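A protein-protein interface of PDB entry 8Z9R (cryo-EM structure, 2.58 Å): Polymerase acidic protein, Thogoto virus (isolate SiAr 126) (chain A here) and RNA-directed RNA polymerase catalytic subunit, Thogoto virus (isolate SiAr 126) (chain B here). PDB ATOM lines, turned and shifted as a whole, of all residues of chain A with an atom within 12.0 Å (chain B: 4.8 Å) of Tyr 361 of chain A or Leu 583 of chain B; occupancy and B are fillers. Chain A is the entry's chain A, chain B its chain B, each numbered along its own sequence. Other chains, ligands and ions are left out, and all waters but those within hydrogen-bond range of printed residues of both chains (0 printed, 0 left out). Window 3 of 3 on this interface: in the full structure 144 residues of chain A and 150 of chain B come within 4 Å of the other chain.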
ATOM      1  N   GLU A 356      -9.831   8.312 -15.869  1.00  0.00           N
ATOM      2  CA  GLU A 356     -10.511   9.423 -15.220  1.00  0.00           C
ATOM      3  C   GLU A 356      -9.839  10.737 -15.592  1.00  0.00           C
ATOM      4  O   GLU A 356      -8.615  10.870 -15.503  1.00  0.00           O
ATOM      5  CB  GLU A 356     -10.508   9.224 -13.707  1.00  0.00           C
ATOM      6  CG  GLU A 356     -11.164  10.343 -12.928  1.00  0.00           C
ATOM      7  CD  GLU A 356     -11.551   9.920 -11.527  1.00  0.00           C
ATOM      8  OE1 GLU A 356     -10.981   8.929 -11.027  1.00  0.00           O
ATOM      9  OE2 GLU A 356     -12.430  10.574 -10.926  1.00  0.00           O
ATOM     10  N   LYS A 357     -10.643  11.707 -16.016  1.00  0.00           N
ATOM     11  CA  LYS A 357     -10.107  12.977 -16.480  1.00  0.00           C
ATOM     12  C   LYS A 357      -9.473  13.754 -15.334  1.00  0.00           C
ATOM     13  O   LYS A 357      -9.909  13.680 -14.183  1.00  0.00           O
ATOM     14  CB  LYS A 357     -11.205  13.821 -17.124  1.00  0.00           C
ATOM     15  CG  LYS A 357     -11.940  13.134 -18.256  1.00  0.00           C
ATOM     16  CD  LYS A 357     -12.786  14.124 -19.035  1.00  0.00           C
ATOM     17  CE  LYS A 357     -13.631  13.422 -20.081  1.00  0.00           C
ATOM     18  NZ  LYS A 357     -12.844  12.412 -20.840  1.00  0.00           N
ATOM     19  N   ASN A 358      -8.428  14.507 -15.663  1.00  0.00           N
ATOM     20  CA  ASN A 358      -7.833  15.413 -14.698  1.00  0.00           C
ATOM     21  C   ASN A 358      -8.753  16.611 -14.475  1.00  0.00           C
ATOM     22  O   ASN A 358      -9.709  16.846 -15.219  1.00  0.00           O
ATOM     23  CB  ASN A 358      -6.462  15.886 -15.177  1.00  0.00           C
ATOM     24  CG  ASN A 358      -5.480  14.749 -15.352  1.00  0.00           C
ATOM     25  OD1 ASN A 358      -4.754  14.692 -16.342  1.00  0.00           O
ATOM     26  ND2 ASN A 358      -5.452  13.837 -14.389  1.00  0.00           N
ATOM     27  N   ALA A 359      -8.456  17.373 -13.430  1.00  0.00           N
ATOM     28  CA  ALA A 359      -9.211  18.587 -13.174  1.00  0.00           C
ATOM     29  C   ALA A 359      -8.924  19.622 -14.257  1.00  0.00           C
ATOM     30  O   ALA A 359      -7.917  19.559 -14.965  1.00  0.00           O
ATOM     31  CB  ALA A 359      -8.873  19.150 -11.796  1.00  0.00           C
ATOM     32  N   ILE A 360      -9.843  20.571 -14.402  1.00  0.00           N
ATOM     33  CA  ILE A 360      -9.706  21.652 -15.370  1.00  0.00           C
ATOM     34  C   ILE A 360      -9.897  22.969 -14.635  1.00  0.00           C
ATOM     35  O   ILE A 360     -10.973  23.225 -14.081  1.00  0.00           O
ATOM     36  CB  ILE A 360     -10.708  21.528 -16.528  1.00  0.00           C
ATOM     37  CG1 ILE A 360     -10.523  20.190 -17.249  1.00  0.00           C
ATOM     38  CG2 ILE A 360     -10.549  22.689 -17.494  1.00  0.00           C
ATOM     39  CD1 ILE A 360     -11.232  20.106 -18.577  1.00  0.00           C
ATOM     40  N   TYR A 361      -8.858  23.799 -14.625  1.00  0.00           N
ATOM     41  CA  TYR A 361      -8.911  25.113 -13.997  1.00  0.00           C
ATOM     42  C   TYR A 361      -8.655  26.236 -14.986  1.00  0.00           C
ATOM     43  O   TYR A 361      -9.397  27.225 -15.001  1.00  0.00           O
ATOM     44  CB  TYR A 361      -7.900  25.187 -12.842  1.00  0.00           C
ATOM     45  CG  TYR A 361      -8.042  24.071 -11.834  1.00  0.00           C
ATOM     46  CD1 TYR A 361      -9.283  23.725 -11.322  1.00  0.00           C
ATOM     47  CD2 TYR A 361      -6.934  23.365 -11.395  1.00  0.00           C
ATOM     48  CE1 TYR A 361      -9.416  22.707 -10.402  1.00  0.00           C
ATOM     49  CE2 TYR A 361      -7.057  22.345 -10.475  1.00  0.00           C
ATOM     50  CZ  TYR A 361      -8.299  22.020  -9.982  1.00  0.00           C
ATOM     51  OH  TYR A 361      -8.424  21.004  -9.067  1.00  0.00           O
ATOM     52  N   THR A 362      -7.626  26.112 -15.818  1.00  0.00           N
ATOM     53  CA  THR A 362      -7.267  27.136 -16.783  1.00  0.00           C
ATOM     54  C   THR A 362      -7.735  26.726 -18.177  1.00  0.00           C
ATOM     55  O   THR A 362      -8.263  25.633 -18.392  1.00  0.00           O
ATOM     56  CB  THR A 362      -5.759  27.381 -16.765  1.00  0.00           C
ATOM     57  OG1 THR A 362      -5.079  26.207 -17.220  1.00  0.00           O
ATOM     58  CG2 THR A 362      -5.293  27.697 -15.359  1.00  0.00           C
ATOM     59  N   GLU A 363      -7.543  27.628 -19.140  1.00  0.00           N
ATOM     60  CA  GLU A 363      -7.879  27.314 -20.524  1.00  0.00           C
ATOM     61  C   GLU A 363      -6.876  26.338 -21.129  1.00  0.00           C
ATOM     62  O   GLU A 363      -7.246  25.504 -21.964  1.00  0.00           O
ATOM     63  CB  GLU A 363      -7.954  28.603 -21.343  1.00  0.00           C
ATOM     64  CG  GLU A 363      -8.076  28.401 -22.841  1.00  0.00           C
ATOM     65  CD  GLU A 363      -8.397  29.690 -23.572  1.00  0.00           C
ATOM     66  OE1 GLU A 363      -9.078  30.554 -22.982  1.00  0.00           O
ATOM     67  OE2 GLU A 363      -7.971  29.838 -24.736  1.00  0.00           O
ATOM     68  N   VAL A 364      -5.610  26.424 -20.713  1.00  0.00           N
ATOM     69  CA  VAL A 364      -4.607  25.449 -21.135  1.00  0.00           C
ATOM     70  C   VAL A 364      -5.017  24.048 -20.701  1.00  0.00           C
ATOM     71  O   VAL A 364      -4.844  23.072 -21.444  1.00  0.00           O
ATOM     72  CB  VAL A 364      -3.227  25.838 -20.573  1.00  0.00           C
ATOM     73  CG1 VAL A 364      -2.273  24.662 -20.625  1.00  0.00           C
ATOM     74  CG2 VAL A 364      -2.658  27.020 -21.331  1.00  0.00           C
ATOM     75  N   ASP A 365      -5.566  23.929 -19.491  1.00  0.00           N
ATOM     76  CA  ASP A 365      -6.049  22.640 -19.013  1.00  0.00           C
ATOM     77  C   ASP A 365      -7.170  22.115 -19.899  1.00  0.00           C
ATOM     78  O   ASP A 365      -7.212  20.922 -20.222  1.00  0.00           O
ATOM     79  CB  ASP A 365      -6.528  22.771 -17.571  1.00  0.00           C
ATOM     80  CG  ASP A 365      -5.427  23.212 -16.638  1.00  0.00           C
ATOM     81  OD1 ASP A 365      -4.307  23.461 -17.123  1.00  0.00           O
ATOM     82  OD2 ASP A 365      -5.679  23.302 -15.420  1.00  0.00           O
ATOM     83  N   GLY A 366      -8.092  22.994 -20.293  1.00  0.00           N
ATOM     84  CA  GLY A 366      -9.160  22.579 -21.186  1.00  0.00           C
ATOM     85  C   GLY A 366      -8.643  22.119 -22.533  1.00  0.00           C
ATOM     86  O   GLY A 366      -9.119  21.125 -23.082  1.00  0.00           O
ATOM     87  N   VAL A 367      -7.653  22.829 -23.079  1.00  0.00           N
ATOM     88  CA  VAL A 367      -7.067  22.431 -24.359  1.00  0.00           C
ATOM     89  C   VAL A 367      -6.417  21.058 -24.240  1.00  0.00           C
ATOM     90  O   VAL A 367      -6.612  20.180 -25.091  1.00  0.00           O
ATOM     91  CB  VAL A 367      -6.059  23.490 -24.839  1.00  0.00           C
ATOM     92  CG1 VAL A 367      -5.352  23.015 -26.095  1.00  0.00           C
ATOM     93  CG2 VAL A 367      -6.760  24.811 -25.092  1.00  0.00           C
ATOM     94  N   ALA A 368      -5.635  20.853 -23.176  1.00  0.00           N
ATOM     95  CA  ALA A 368      -4.952  19.576 -22.995  1.00  0.00           C
ATOM     96  C   ALA A 368      -5.947  18.434 -22.831  1.00  0.00           C
ATOM     97  O   ALA A 368      -5.788  17.370 -23.444  1.00  0.00           O
ATOM     98  CB  ALA A 368      -4.018  19.649 -21.788  1.00  0.00           C
ATOM     99  N   GLU A 369      -6.986  18.636 -22.020  1.00  0.00           N
ATOM    100  CA  GLU A 369      -7.958  17.572 -21.808  1.00  0.00           C
ATOM    101  C   GLU A 369      -8.790  17.311 -23.055  1.00  0.00           C
ATOM    102  O   GLU A 369      -9.160  16.164 -23.315  1.00  0.00           O
ATOM    103  CB  GLU A 369      -8.852  17.900 -20.616  1.00  0.00           C
ATOM    104  CG  GLU A 369      -8.110  17.876 -19.296  1.00  0.00           C
ATOM    105  CD  GLU A 369      -7.562  16.502 -18.963  1.00  0.00           C
ATOM    106  OE1 GLU A 369      -8.165  15.494 -19.388  1.00  0.00           O
ATOM    107  OE2 GLU A 369      -6.514  16.428 -18.289  1.00  0.00           O
ATOM    108  N   GLY A 370      -9.085  18.347 -23.842  1.00  0.00           N
ATOM    109  CA  GLY A 370      -9.763  18.123 -25.108  1.00  0.00           C
ATOM    110  C   GLY A 370      -8.919  17.318 -26.076  1.00  0.00           C
ATOM    111  O   GLY A 370      -9.426  16.431 -26.766  1.00  0.00           O
ATOM    112  N   VAL B 566      -7.442  16.172  -8.174  1.00  0.00           N
ATOM    113  CA  VAL B 566      -7.445  17.597  -7.871  1.00  0.00           C
ATOM    114  C   VAL B 566      -6.373  18.260  -8.721  1.00  0.00           C
ATOM    115  O   VAL B 566      -6.470  19.447  -9.055  1.00  0.00           O
ATOM    116  CB  VAL B 566      -7.223  17.860  -6.369  1.00  0.00           C
ATOM    117  CG1 VAL B 566      -5.835  17.413  -5.937  1.00  0.00           C
ATOM    118  CG2 VAL B 566      -7.442  19.328  -6.045  1.00  0.00           C
ATOM    119  N   HIS B 567      -5.352  17.495  -9.089  1.00  0.00           N
ATOM    120  CA  HIS B 567      -4.269  18.021  -9.901  1.00  0.00           C
ATOM    121  C   HIS B 567      -4.700  18.138 -11.353  1.00  0.00           C
ATOM    122  O   HIS B 567      -5.434  17.295 -11.873  1.00  0.00           O
ATOM    123  CB  HIS B 567      -3.034  17.129  -9.796  1.00  0.00           C
ATOM    124  CG  HIS B 567      -2.306  17.265  -8.498  1.00  0.00           C
ATOM    125  ND1 HIS B 567      -2.491  16.395  -7.447  1.00  0.00           N
ATOM    126  CD2 HIS B 567      -1.394  18.174  -8.079  1.00  0.00           C
ATOM    127  CE1 HIS B 567      -1.721  16.758  -6.438  1.00  0.00           C
ATOM    128  NE2 HIS B 567      -1.045  17.835  -6.795  1.00  0.00           N
ATOM    129  N   SER B 568      -4.238  19.195 -12.001  1.00  0.00           N
ATOM    130  CA  SER B 568      -4.503  19.450 -13.404  1.00  0.00           C
ATOM    131  C   SER B 568      -3.172  19.618 -14.129  1.00  0.00           C
ATOM    132  O   SER B 568      -2.100  19.495 -13.534  1.00  0.00           O
ATOM    133  CB  SER B 568      -5.388  20.686 -13.565  1.00  0.00           C
ATOM    134  OG  SER B 568      -5.635  20.944 -14.930  1.00  0.00           O
ATOM    135  N   THR B 571      -1.506  22.522 -12.681  1.00  0.00           N
ATOM    136  CA  THR B 571      -1.271  22.369 -11.252  1.00  0.00           C
ATOM    137  C   THR B 571      -0.462  21.114 -10.933  1.00  0.00           C
ATOM    138  O   THR B 571      -0.680  20.478  -9.901  1.00  0.00           O
ATOM    139  CB  THR B 571      -2.594  22.354 -10.489  1.00  0.00           C
ATOM    140  OG1 THR B 571      -3.382  21.237 -10.915  1.00  0.00           O
ATOM    141  CG2 THR B 571      -3.366  23.630 -10.747  1.00  0.00           C
ATOM    142  N   LEU B 579      -3.658  22.329  -2.266  1.00  0.00           N
ATOM    143  CA  LEU B 579      -4.598  22.658  -3.333  1.00  0.00           C
ATOM    144  C   LEU B 579      -6.025  22.285  -2.948  1.00  0.00           C
ATOM    145  O   LEU B 579      -6.964  23.044  -3.215  1.00  0.00           O
ATOM    146  CB  LEU B 579      -4.181  21.955  -4.623  1.00  0.00           C
ATOM    147  CG  LEU B 579      -5.029  22.186  -5.872  1.00  0.00           C
ATOM    148  CD1 LEU B 579      -5.119  23.667  -6.189  1.00  0.00           C
ATOM    149  CD2 LEU B 579      -4.444  21.423  -7.045  1.00  0.00           C
ATOM    150  N   ARG B 580      -6.208  21.121  -2.319  1.00  0.00           N
ATOM    151  CA  ARG B 580      -7.539  20.719  -1.880  1.00  0.00           C
ATOM    152  C   ARG B 580      -8.071  21.652  -0.802  1.00  0.00           C
ATOM    153  O   ARG B 580      -9.265  21.975  -0.789  1.00  0.00           O
ATOM    154  CB  ARG B 580      -7.516  19.276  -1.380  1.00  0.00           C
ATOM    155  CG  ARG B 580      -7.290  18.254  -2.472  1.00  0.00           C
ATOM    156  CD  ARG B 580      -7.541  16.842  -1.982  1.00  0.00           C
ATOM    157  NE  ARG B 580      -7.468  15.877  -3.072  1.00  0.00           N
ATOM    158  CZ  ARG B 580      -8.469  15.600  -3.896  1.00  0.00           C
ATOM    159  NH1 ARG B 580      -9.645  16.190  -3.777  1.00  0.00           N
ATOM    160  NH2 ARG B 580      -8.281  14.710  -4.866  1.00  0.00           N
ATOM    161  N   ARG B 581      -7.209  22.084   0.120  1.00  0.00           N
ATOM    162  CA  ARG B 581      -7.635  23.046   1.131  1.00  0.00           C
ATOM    163  C   ARG B 581      -8.039  24.369   0.495  1.00  0.00           C
ATOM    164  O   ARG B 581      -9.048  24.970   0.880  1.00  0.00           O
ATOM    165  CB  ARG B 581      -6.521  23.264   2.154  1.00  0.00           C
ATOM    166  CG  ARG B 581      -6.804  24.389   3.133  1.00  0.00           C
ATOM    167  CD  ARG B 581      -5.542  24.855   3.830  1.00  0.00           C
ATOM    168  NE  ARG B 581      -5.831  25.419   5.143  1.00  0.00           N
ATOM    169  CZ  ARG B 581      -4.935  26.020   5.913  1.00  0.00           C
ATOM    170  NH1 ARG B 581      -3.678  26.162   5.529  1.00  0.00           N
ATOM    171  NH2 ARG B 581      -5.311  26.491   7.098  1.00  0.00           N
ATOM    172  N   HIS B 582      -7.262  24.838  -0.483  1.00  0.00           N
ATOM    173  CA  HIS B 582      -7.585  26.099  -1.142  1.00  0.00           C
ATOM    174  C   HIS B 582      -8.901  26.004  -1.902  1.00  0.00           C
ATOM    175  O   HIS B 582      -9.703  26.945  -1.888  1.00  0.00           O
ATOM    176  CB  HIS B 582      -6.454  26.504  -2.082  1.00  0.00           C
ATOM    177  CG  HIS B 582      -6.752  27.726  -2.893  1.00  0.00           C
ATOM    178  ND1 HIS B 582      -6.522  29.002  -2.424  1.00  0.00           N
ATOM    179  CD2 HIS B 582      -7.270  27.868  -4.134  1.00  0.00           C
ATOM    180  CE1 HIS B 582      -6.881  29.877  -3.346  1.00  0.00           C
ATOM    181  NE2 HIS B 582      -7.338  29.215  -4.394  1.00  0.00           N
ATOM    182  N   LEU B 583      -9.141  24.881  -2.572  1.00  0.00           N
ATOM    183  CA  LEU B 583     -10.357  24.709  -3.356  1.00  0.00           C
ATOM    184  C   LEU B 583     -11.560  24.304  -2.516  1.00  0.00           C
ATOM    185  O   LEU B 583     -12.667  24.212  -3.055  1.00  0.00           O
ATOM    186  CB  LEU B 583     -10.129  23.675  -4.460  1.00  0.00           C
ATOM    187  CG  LEU B 583      -9.161  24.094  -5.566  1.00  0.00           C
ATOM    188  CD1 LEU B 583      -8.957  22.958  -6.547  1.00  0.00           C
ATOM    189  CD2 LEU B 583      -9.665  25.336  -6.276  1.00  0.00           C
ATOM    190  N   GLY B 584     -11.377  24.058  -1.222  1.00  0.00           N
ATOM    191  CA  GLY B 584     -12.470  23.657  -0.363  1.00  0.00           C
ATOM    192  C   GLY B 584     -12.830  22.191  -0.423  1.00  0.00           C
ATOM    193  O   GLY B 584     -13.792  21.781   0.238  1.00  0.00           O
ATOM    194  N   LEU B 585     -12.097  21.388  -1.193  1.00  0.00           N
ATOM    195  CA  LEU B 585     -12.370  19.959  -1.279  1.00  0.00           C
ATOM    196  C   LEU B 585     -11.958  19.207  -0.022  1.00  0.00           C
ATOM    197  O   LEU B 585     -12.335  18.040   0.131  1.00  0.00           O
ATOM    198  CB  LEU B 585     -11.654  19.367  -2.494  1.00  0.00           C
ATOM    199  CG  LEU B 585     -11.943  20.050  -3.830  1.00  0.00           C
ATOM    200  CD1 LEU B 585     -10.921  19.638  -4.871  1.00  0.00           C
ATOM    201  CD2 LEU B 585     -13.349  19.726  -4.299  1.00  0.00           C
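Printed residues of chain A that touch a printed residue of chain B: Asn 358, Ala 359, Tyr 361 and Asp 365. Hydrophobic or aromatic side chains of chain A within 4 Å of the printed part of chain B: Ala 359 and Tyr 361. Among the printed residues, 9 pairs touch across the chains. Among the printed residues, no Asp or Glu carboxylate lies within 4 Å of a Lys or Arg side-chain nitrogen of the other chain.
Lys 357 of chain A touches none of the printed residues of chain B. Tyr 361 of chain A touches just these residues of chain B: Val 566 (2.5 Å), Ser 568 (3.8 Å), Thr 571 (3.6 Å) and Leu 583 (3.2 Å). Val 364 of chain A touches none of the printed residues of chain B. Of the printed residues of chain B, Asp 365 of chain A touches Ser 568 (2.4 Å). Of the printed residues of chain A, His 567 of chain B touches Asn 358 and Ala 359. Of chain A, only Tyr 361 (3.6 Å) comes within 4 Å of Thr 571 of chain B. No residue of chain A comes within 4 Å of Leu 579 of chain B. No residue of chain A comes within 4 Å of His 582 of chain B. Of chain A, only Tyr 361 (3.2 Å) comes within 4 Å of Leu 583 of chain B. No residue of chain A comes within 4 Å of Gly 584 of chain B. No residue of chain A comes within 4 Å of Leu 585 of chain B. The nearest residue of chain A that does not touch Leu 583 of chain B is Ala 359 of chain A (6.5 Å). The nearest printed residue of chain A that does not touch His 567 of chain B is Tyr 361 of chain A (4.7 Å).
The side-chain hydroxyl of Thr 571 of chain B lies within hydrogen-bond range of the backbone NH of Ser 568 of chain B (2.5 Å). The backbone NH of Tyr 361 of chain A is in hydrogen-bond range of the side-chain carboxylate of Asp 365 of chain A, 3.3 Å away. OG1 of Thr 362 of chain A is in hydrogen-bond range of OD1 of Asp 365 of chain A (2.9 Å). The side-chain carboxylate (OE2) of Glu 369 of chain A sits close to the side-chain amide oxygen (OD1) of Asn 358 of chain A (3.1 Å).
The side-chain hydroxyl (OH) of Tyr 361 of chain A is in hydrogen-bond range of the backbone carbonyl oxygen (O) of Val 566 of chain B (2.5 Å). The backbone NH (N) of Ala 359 of chain A sits at hydrogen-bond distance from the backbone carbonyl oxygen (O) of His 567 of chain B (3.4 Å). O of Ala 359 of chain A is in hydrogen-bond range of OG of Ser 568 of chain B. The side-chain hydroxyl of Ser 568 of chain B sits at hydrogen-bond distance from the side-chain carboxylate of Asp 365 of chain A.
Among the printed residues, merely in contact across the chains: Asn 358 of chain A with His 567 of chain B (3.7 Å), Ala 359 of chain A with Val 566 of chain B (3.7 Å), Tyr 361 of chain A with Ser 568 of chain B (3.8 Å), Tyr 361 of chain A with Thr 571 of chain B (3.6 Å) and Tyr 361 of chain A with Leu 583 of chain B (3.2 Å).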
